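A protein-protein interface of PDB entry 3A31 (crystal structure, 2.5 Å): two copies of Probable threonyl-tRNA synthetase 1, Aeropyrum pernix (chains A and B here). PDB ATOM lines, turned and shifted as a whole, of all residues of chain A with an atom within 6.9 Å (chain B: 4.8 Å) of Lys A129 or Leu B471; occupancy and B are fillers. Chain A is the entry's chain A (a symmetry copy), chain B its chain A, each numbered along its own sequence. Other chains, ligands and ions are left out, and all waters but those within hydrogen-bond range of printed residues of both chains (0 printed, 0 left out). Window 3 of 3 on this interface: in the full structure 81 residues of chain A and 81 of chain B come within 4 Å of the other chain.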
ATOM      1  N   LYS A 125      29.084  -9.480  -7.852  1.00  0.00           N
ATOM      2  CA  LYS A 125      28.121  -9.303  -6.773  1.00  0.00           C
ATOM      3  C   LYS A 125      28.659  -9.730  -5.394  1.00  0.00           C
ATOM      4  O   LYS A 125      28.223  -9.190  -4.387  1.00  0.00           O
ATOM      5  CB  LYS A 125      26.866 -10.073  -7.115  1.00  0.00           C
ATOM      6  CG  LYS A 125      26.266  -9.626  -8.475  1.00  0.00           C
ATOM      7  CD  LYS A 125      25.176 -10.536  -9.018  1.00  0.00           C
ATOM      8  CE  LYS A 125      24.225 -10.982  -7.917  1.00  0.00           C
ATOM      9  NZ  LYS A 125      22.923 -11.572  -8.362  1.00  0.00           N
ATOM     10  N   HIS A 126      29.586 -10.697  -5.325  1.00  0.00           N
ATOM     11  CA  HIS A 126      29.930 -11.335  -4.050  1.00  0.00           C
ATOM     12  C   HIS A 126      31.401 -11.331  -3.788  1.00  0.00           C
ATOM     13  O   HIS A 126      31.842 -11.709  -2.692  1.00  0.00           O
ATOM     14  CB  HIS A 126      29.305 -12.745  -3.914  1.00  0.00           C
ATOM     15  CG  HIS A 126      27.825 -12.762  -4.211  1.00  0.00           C
ATOM     16  ND1 HIS A 126      26.890 -12.168  -3.389  1.00  0.00           N
ATOM     17  CD2 HIS A 126      27.135 -13.210  -5.292  1.00  0.00           C
ATOM     18  CE1 HIS A 126      25.693 -12.268  -3.930  1.00  0.00           C
ATOM     19  NE2 HIS A 126      25.814 -12.898  -5.084  1.00  0.00           N
ATOM     20  N   ARG A 127      32.163 -10.829  -4.760  1.00  0.00           N
ATOM     21  CA  ARG A 127      33.639 -10.817  -4.722  1.00  0.00           C
ATOM     22  C   ARG A 127      34.169 -12.083  -4.100  1.00  0.00           C
ATOM     23  O   ARG A 127      33.779 -13.192  -4.502  1.00  0.00           O
ATOM     24  CB  ARG A 127      34.190  -9.578  -4.021  1.00  0.00           C
ATOM     25  CG  ARG A 127      33.299  -8.368  -4.211  1.00  0.00           C
ATOM     26  CD  ARG A 127      34.008  -7.021  -4.276  1.00  0.00           C
ATOM     27  NE  ARG A 127      33.230  -6.206  -5.221  1.00  0.00           N
ATOM     28  CZ  ARG A 127      33.406  -6.193  -6.553  1.00  0.00           C
ATOM     29  NH1 ARG A 127      34.378  -6.904  -7.131  1.00  0.00           N
ATOM     30  NH2 ARG A 127      32.614  -5.453  -7.323  1.00  0.00           N
ATOM     31  N   SER A 128      35.011 -11.931  -3.089  1.00  0.00           N
ATOM     32  CA  SER A 128      35.763 -13.084  -2.584  1.00  0.00           C
ATOM     33  C   SER A 128      34.947 -14.074  -1.773  1.00  0.00           C
ATOM     34  O   SER A 128      35.498 -15.110  -1.371  1.00  0.00           O
ATOM     35  CB  SER A 128      37.034 -12.676  -1.819  1.00  0.00           C
ATOM     36  OG  SER A 128      36.700 -11.682  -0.880  1.00  0.00           O
ATOM     37  N   LYS A 129      33.665 -13.774  -1.522  1.00  0.00           N
ATOM     38  CA  LYS A 129      32.769 -14.726  -0.810  1.00  0.00           C
ATOM     39  C   LYS A 129      32.469 -15.954  -1.665  1.00  0.00           C
ATOM     40  O   LYS A 129      32.099 -17.001  -1.151  1.00  0.00           O
ATOM     41  CB  LYS A 129      31.437 -14.087  -0.436  1.00  0.00           C
ATOM     42  CG  LYS A 129      31.487 -13.000   0.599  1.00  0.00           C
ATOM     43  CD  LYS A 129      30.183 -13.010   1.350  1.00  0.00           C
ATOM     44  CE  LYS A 129      29.121 -12.149   0.685  1.00  0.00           C
ATOM     45  NZ  LYS A 129      27.838 -12.277   1.508  1.00  0.00           N
ATOM     46  N   LEU A 130      32.599 -15.791  -2.984  1.00  0.00           N
ATOM     47  CA  LEU A 130      32.519 -16.889  -3.916  1.00  0.00           C
ATOM     48  C   LEU A 130      33.602 -17.929  -3.614  1.00  0.00           C
ATOM     49  O   LEU A 130      34.785 -17.604  -3.597  1.00  0.00           O
ATOM     50  CB  LEU A 130      32.716 -16.341  -5.302  1.00  0.00           C
ATOM     51  CG  LEU A 130      32.177 -17.240  -6.396  1.00  0.00           C
ATOM     52  CD1 LEU A 130      30.620 -17.560  -6.218  1.00  0.00           C
ATOM     53  CD2 LEU A 130      32.464 -16.576  -7.694  1.00  0.00           C
ATOM     54  N   PRO A 131      33.219 -19.167  -3.313  1.00  0.00           N
ATOM     55  CA  PRO A 131      34.261 -20.197  -3.115  1.00  0.00           C
ATOM     56  C   PRO A 131      35.063 -20.573  -4.389  1.00  0.00           C
ATOM     57  O   PRO A 131      34.563 -20.430  -5.510  1.00  0.00           O
ATOM     58  CB  PRO A 131      33.464 -21.414  -2.625  1.00  0.00           C
ATOM     59  CG  PRO A 131      32.139 -20.827  -2.095  1.00  0.00           C
ATOM     60  CD  PRO A 131      31.873 -19.695  -3.074  1.00  0.00           C
ATOM     61  N   LEU A 132      36.303 -21.021  -4.186  1.00  0.00           N
ATOM     62  CA  LEU A 132      37.152 -21.604  -5.211  1.00  0.00           C
ATOM     63  C   LEU A 132      37.639 -22.931  -4.668  1.00  0.00           C
ATOM     64  O   LEU A 132      37.957 -23.034  -3.499  1.00  0.00           O
ATOM     65  CB  LEU A 132      38.336 -20.685  -5.468  1.00  0.00           C
ATOM     66  CG  LEU A 132      38.069 -19.295  -6.060  1.00  0.00           C
ATOM     67  CD1 LEU A 132      39.390 -18.595  -6.461  1.00  0.00           C
ATOM     68  CD2 LEU A 132      37.030 -19.261  -7.260  1.00  0.00           C
ATOM     69  N   GLU A 300      40.713  -9.886  -6.687  1.00  0.00           N
ATOM     70  CA  GLU A 300      39.647 -10.193  -5.742  1.00  0.00           C
ATOM     71  C   GLU A 300      39.960 -11.268  -4.696  1.00  0.00           C
ATOM     72  O   GLU A 300      39.377 -11.250  -3.583  1.00  0.00           O
ATOM     73  CB  GLU A 300      38.372 -10.579  -6.491  1.00  0.00           C
ATOM     74  CG  GLU A 300      37.826  -9.486  -7.398  1.00  0.00           C
ATOM     75  CD  GLU A 300      37.398  -8.237  -6.652  1.00  0.00           C
ATOM     76  OE1 GLU A 300      37.223  -8.277  -5.392  1.00  0.00           O
ATOM     77  OE2 GLU A 300      37.223  -7.200  -7.347  1.00  0.00           O
ATOM     78  N   PHE A 301      40.814 -12.231  -5.037  1.00  0.00           N
ATOM     79  CA  PHE A 301      41.083 -13.340  -4.097  1.00  0.00           C
ATOM     80  C   PHE A 301      42.519 -13.364  -3.601  1.00  0.00           C
ATOM     81  O   PHE A 301      42.857 -14.146  -2.726  1.00  0.00           O
ATOM     82  CB  PHE A 301      40.745 -14.713  -4.705  1.00  0.00           C
ATOM     83  CG  PHE A 301      39.323 -14.869  -5.144  1.00  0.00           C
ATOM     84  CD1 PHE A 301      38.423 -15.561  -4.368  1.00  0.00           C
ATOM     85  CD2 PHE A 301      38.888 -14.319  -6.350  1.00  0.00           C
ATOM     86  CE1 PHE A 301      37.077 -15.705  -4.791  1.00  0.00           C
ATOM     87  CE2 PHE A 301      37.568 -14.456  -6.778  1.00  0.00           C
ATOM     88  CZ  PHE A 301      36.655 -15.166  -6.001  1.00  0.00           C
ATOM     89  N   ILE B 339      17.079 -20.574  -3.086  1.00  0.00           N
ATOM     90  CA  ILE B 339      17.553 -21.015  -1.758  1.00  0.00           C
ATOM     91  C   ILE B 339      16.378 -21.616  -1.003  1.00  0.00           C
ATOM     92  O   ILE B 339      15.391 -20.918  -0.743  1.00  0.00           O
ATOM     93  CB  ILE B 339      18.126 -19.823  -0.941  1.00  0.00           C
ATOM     94  CG1 ILE B 339      19.409 -19.304  -1.611  1.00  0.00           C
ATOM     95  CG2 ILE B 339      18.403 -20.234   0.521  1.00  0.00           C
ATOM     96  CD1 ILE B 339      20.045 -17.987  -0.966  1.00  0.00           C
ATOM     97  N   ALA B 342      17.508 -21.313   4.496  1.00  0.00           N
ATOM     98  CA  ALA B 342      18.558 -20.409   4.949  1.00  0.00           C
ATOM     99  C   ALA B 342      18.784 -20.729   6.424  1.00  0.00           C
ATOM    100  O   ALA B 342      17.824 -20.635   7.220  1.00  0.00           O
ATOM    101  CB  ALA B 342      18.156 -18.974   4.782  1.00  0.00           C
ATOM    102  N   ALA B 375      21.717 -22.168   2.223  1.00  0.00           N
ATOM    103  CA  ALA B 375      22.623 -21.055   2.444  1.00  0.00           C
ATOM    104  C   ALA B 375      22.804 -20.833   3.961  1.00  0.00           C
ATOM    105  O   ALA B 375      21.816 -20.675   4.705  1.00  0.00           O
ATOM    106  CB  ALA B 375      22.129 -19.805   1.755  1.00  0.00           C
ATOM    107  N   VAL B 376      24.054 -20.864   4.419  1.00  0.00           N
ATOM    108  CA  VAL B 376      24.326 -20.590   5.830  1.00  0.00           C
ATOM    109  C   VAL B 376      24.744 -19.132   5.953  1.00  0.00           C
ATOM    110  O   VAL B 376      25.562 -18.687   5.167  1.00  0.00           O
ATOM    111  CB  VAL B 376      25.457 -21.444   6.372  1.00  0.00           C
ATOM    112  CG1 VAL B 376      25.893 -20.919   7.743  1.00  0.00           C
ATOM    113  CG2 VAL B 376      25.016 -22.874   6.473  1.00  0.00           C
ATOM    114  N   LYS B 377      24.198 -18.417   6.926  1.00  0.00           N
ATOM    115  CA  LYS B 377      24.586 -17.021   7.225  1.00  0.00           C
ATOM    116  C   LYS B 377      25.028 -16.861   8.730  1.00  0.00           C
ATOM    117  O   LYS B 377      24.295 -17.253   9.673  1.00  0.00           O
ATOM    118  CB  LYS B 377      23.421 -16.089   6.908  1.00  0.00           C
ATOM    119  CG  LYS B 377      23.574 -14.604   7.394  1.00  0.00           C
ATOM    120  CD  LYS B 377      24.796 -13.884   6.739  1.00  0.00           C
ATOM    121  CE  LYS B 377      24.712 -12.357   6.885  1.00  0.00           C
ATOM    122  NZ  LYS B 377      25.534 -11.657   5.797  1.00  0.00           N
ATOM    123  N   ILE B 391      18.422 -10.203   3.869  1.00  0.00           N
ATOM    124  CA  ILE B 391      17.963 -11.456   3.347  1.00  0.00           C
ATOM    125  C   ILE B 391      16.509 -11.430   2.768  1.00  0.00           C
ATOM    126  O   ILE B 391      16.248 -12.002   1.698  1.00  0.00           O
ATOM    127  CB  ILE B 391      18.131 -12.527   4.428  1.00  0.00           C
ATOM    128  CG1 ILE B 391      19.628 -12.854   4.673  1.00  0.00           C
ATOM    129  CG2 ILE B 391      17.332 -13.778   4.073  1.00  0.00           C
ATOM    130  CD1 ILE B 391      19.850 -13.593   5.968  1.00  0.00           C
ATOM    131  N   ALA B 395      17.414 -12.191  -1.036  1.00  0.00           N
ATOM    132  CA  ALA B 395      17.501 -13.598  -1.302  1.00  0.00           C
ATOM    133  C   ALA B 395      16.172 -14.361  -1.162  1.00  0.00           C
ATOM    134  O   ALA B 395      15.983 -15.397  -1.847  1.00  0.00           O
ATOM    135  CB  ALA B 395      18.524 -14.199  -0.453  1.00  0.00           C
ATOM    136  N   PHE B 467      24.406 -22.184  -1.412  1.00  0.00           N
ATOM    137  CA  PHE B 467      24.433 -20.807  -1.850  1.00  0.00           C
ATOM    138  C   PHE B 467      24.807 -19.838  -0.697  1.00  0.00           C
ATOM    139  O   PHE B 467      24.408 -18.661  -0.704  1.00  0.00           O
ATOM    140  CB  PHE B 467      23.091 -20.409  -2.470  1.00  0.00           C
ATOM    141  CG  PHE B 467      22.819 -20.998  -3.825  1.00  0.00           C
ATOM    142  CD1 PHE B 467      23.851 -21.161  -4.772  1.00  0.00           C
ATOM    143  CD2 PHE B 467      21.498 -21.284  -4.199  1.00  0.00           C
ATOM    144  CE1 PHE B 467      23.586 -21.678  -6.050  1.00  0.00           C
ATOM    145  CE2 PHE B 467      21.211 -21.750  -5.485  1.00  0.00           C
ATOM    146  CZ  PHE B 467      22.275 -21.976  -6.419  1.00  0.00           C
ATOM    147  N   SER B 468      25.580 -20.328   0.268  1.00  0.00           N
ATOM    148  CA  SER B 468      26.047 -19.481   1.375  1.00  0.00           C
ATOM    149  C   SER B 468      26.597 -18.143   0.940  1.00  0.00           C
ATOM    150  O   SER B 468      26.363 -17.172   1.599  1.00  0.00           O
ATOM    151  CB  SER B 468      27.081 -20.205   2.256  1.00  0.00           C
ATOM    152  OG  SER B 468      26.494 -21.326   2.904  1.00  0.00           O
ATOM    153  N   PHE B 469      27.319 -18.110  -0.170  1.00  0.00           N
ATOM    154  CA  PHE B 469      27.989 -16.898  -0.638  1.00  0.00           C
ATOM    155  C   PHE B 469      27.044 -15.756  -0.990  1.00  0.00           C
ATOM    156  O   PHE B 469      27.487 -14.591  -1.091  1.00  0.00           O
ATOM    157  CB  PHE B 469      28.912 -17.210  -1.821  1.00  0.00           C
ATOM    158  CG  PHE B 469      28.191 -17.655  -3.065  1.00  0.00           C
ATOM    159  CD1 PHE B 469      27.722 -16.706  -3.998  1.00  0.00           C
ATOM    160  CD2 PHE B 469      28.009 -19.012  -3.332  1.00  0.00           C
ATOM    161  CE1 PHE B 469      27.083 -17.107  -5.165  1.00  0.00           C
ATOM    162  CE2 PHE B 469      27.319 -19.447  -4.534  1.00  0.00           C
ATOM    163  CZ  PHE B 469      26.859 -18.488  -5.428  1.00  0.00           C
ATOM    164  N   MET B 470      25.757 -16.102  -1.190  1.00  0.00           N
ATOM    165  CA  MET B 470      24.724 -15.157  -1.584  1.00  0.00           C
ATOM    166  C   MET B 470      24.155 -14.433  -0.391  1.00  0.00           C
ATOM    167  O   MET B 470      23.523 -13.371  -0.533  1.00  0.00           O
ATOM    168  CB  MET B 470      23.569 -15.875  -2.256  1.00  0.00           C
ATOM    169  CG  MET B 470      23.821 -16.233  -3.694  1.00  0.00           C
ATOM    170  SD  MET B 470      22.257 -17.174  -4.438  1.00  0.00           S
ATOM    171  CE  MET B 470      23.085 -17.792  -6.089  1.00  0.00           C
ATOM    172  N   LEU B 471      24.309 -15.032   0.783  1.00  0.00           N
ATOM    173  CA  LEU B 471      23.907 -14.343   1.979  1.00  0.00           C
ATOM    174  C   LEU B 471      25.154 -13.727   2.624  1.00  0.00           C
ATOM    175  O   LEU B 471      25.010 -12.712   3.301  1.00  0.00           O
ATOM    176  CB  LEU B 471      23.201 -15.269   2.951  1.00  0.00           C
ATOM    177  CG  LEU B 471      21.995 -16.092   2.555  1.00  0.00           C
ATOM    178  CD1 LEU B 471      21.441 -16.698   3.794  1.00  0.00           C
ATOM    179  CD2 LEU B 471      20.966 -15.321   1.846  1.00  0.00           C
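O of Phe B469 is in hydrogen-bond range of ND1 of His A126 (3.4 Å). The backbone carbonyl oxygen (O) of Phe B469 sits close to the side-chain amino group (NZ) of Lys A129 (3.5 Å). NZ of Lys A129 sits close to O of Leu B471 (3.4 Å).
NZ of Lys B377 is in hydrogen-bond range of O of Leu B471.
Met B470 touches His A126 (CA to CE1, 3.8 Å). Leu A130 touches Phe B469 (CD1 to CE1, 3.7 Å). CD of Pro A131 touches CD2 of Phe B469, 3.9 Å away.
Lys A129 touches just these residues of chain B: Phe B469 (3.3 Å) and Leu B471 (3.2 Å). Of chain A, only Lys A129 comes within 4 Å of Leu B471. Printed residues of chain B within 4 Å of Leu A130: Phe B469. Of the printed residues of chain A, Phe B469 touches His A126 (3.4 Å), Lys A129 (3.3 Å), Leu A130 (3.7 Å) and Pro A131 (3.9 Å). Of the printed residues of chain B, Pro A131 touches Phe B469 (3.9 Å). Printed residues of chain B within 4 Å of His A126: Phe B469 (3.4 Å) and Met B470 (3.8 Å). Printed residues of chain A within 4 Å of Met B470: His A126 (3.8 Å). Ala B375 touches none of the printed residues of chain A. Ala B395 touches none of the printed residues of chain A. The nearest residue of chain A that does not touch Leu B471 is His A126 (5.6 Å). The nearest printed residue of chain B that does not touch Pro A131 is Ser B468 (6.7 Å).
Of the 12 printed residues of chain B, 3 touch a printed residue of chain A. Hydrophobic or aromatic side chains of chain B that line the printed part of chain A: Phe B469. Along chain B the printed residues that touch a printed residue of chain A span positions 469 to 471. Of the 10 printed residues of chain A, 4 touch a printed residue of chain B. Printed residues of chain A that touch a printed residue of chain B: His A126, Lys A129, Leu A130 and Pro A131. Hydrophobic or aromatic side chains of chain A that line the printed part of chain B: His A126, Leu A130 and Pro A131. Among the printed residues, no Asp or Glu carboxylate lies within 4 Å of a Lys or Arg side-chain nitrogen of the other chain.
No position is printed for both chains. Of the 6 pairs that touch across the chains among the printed residues, none has its exchanged pair printed and touching as well.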
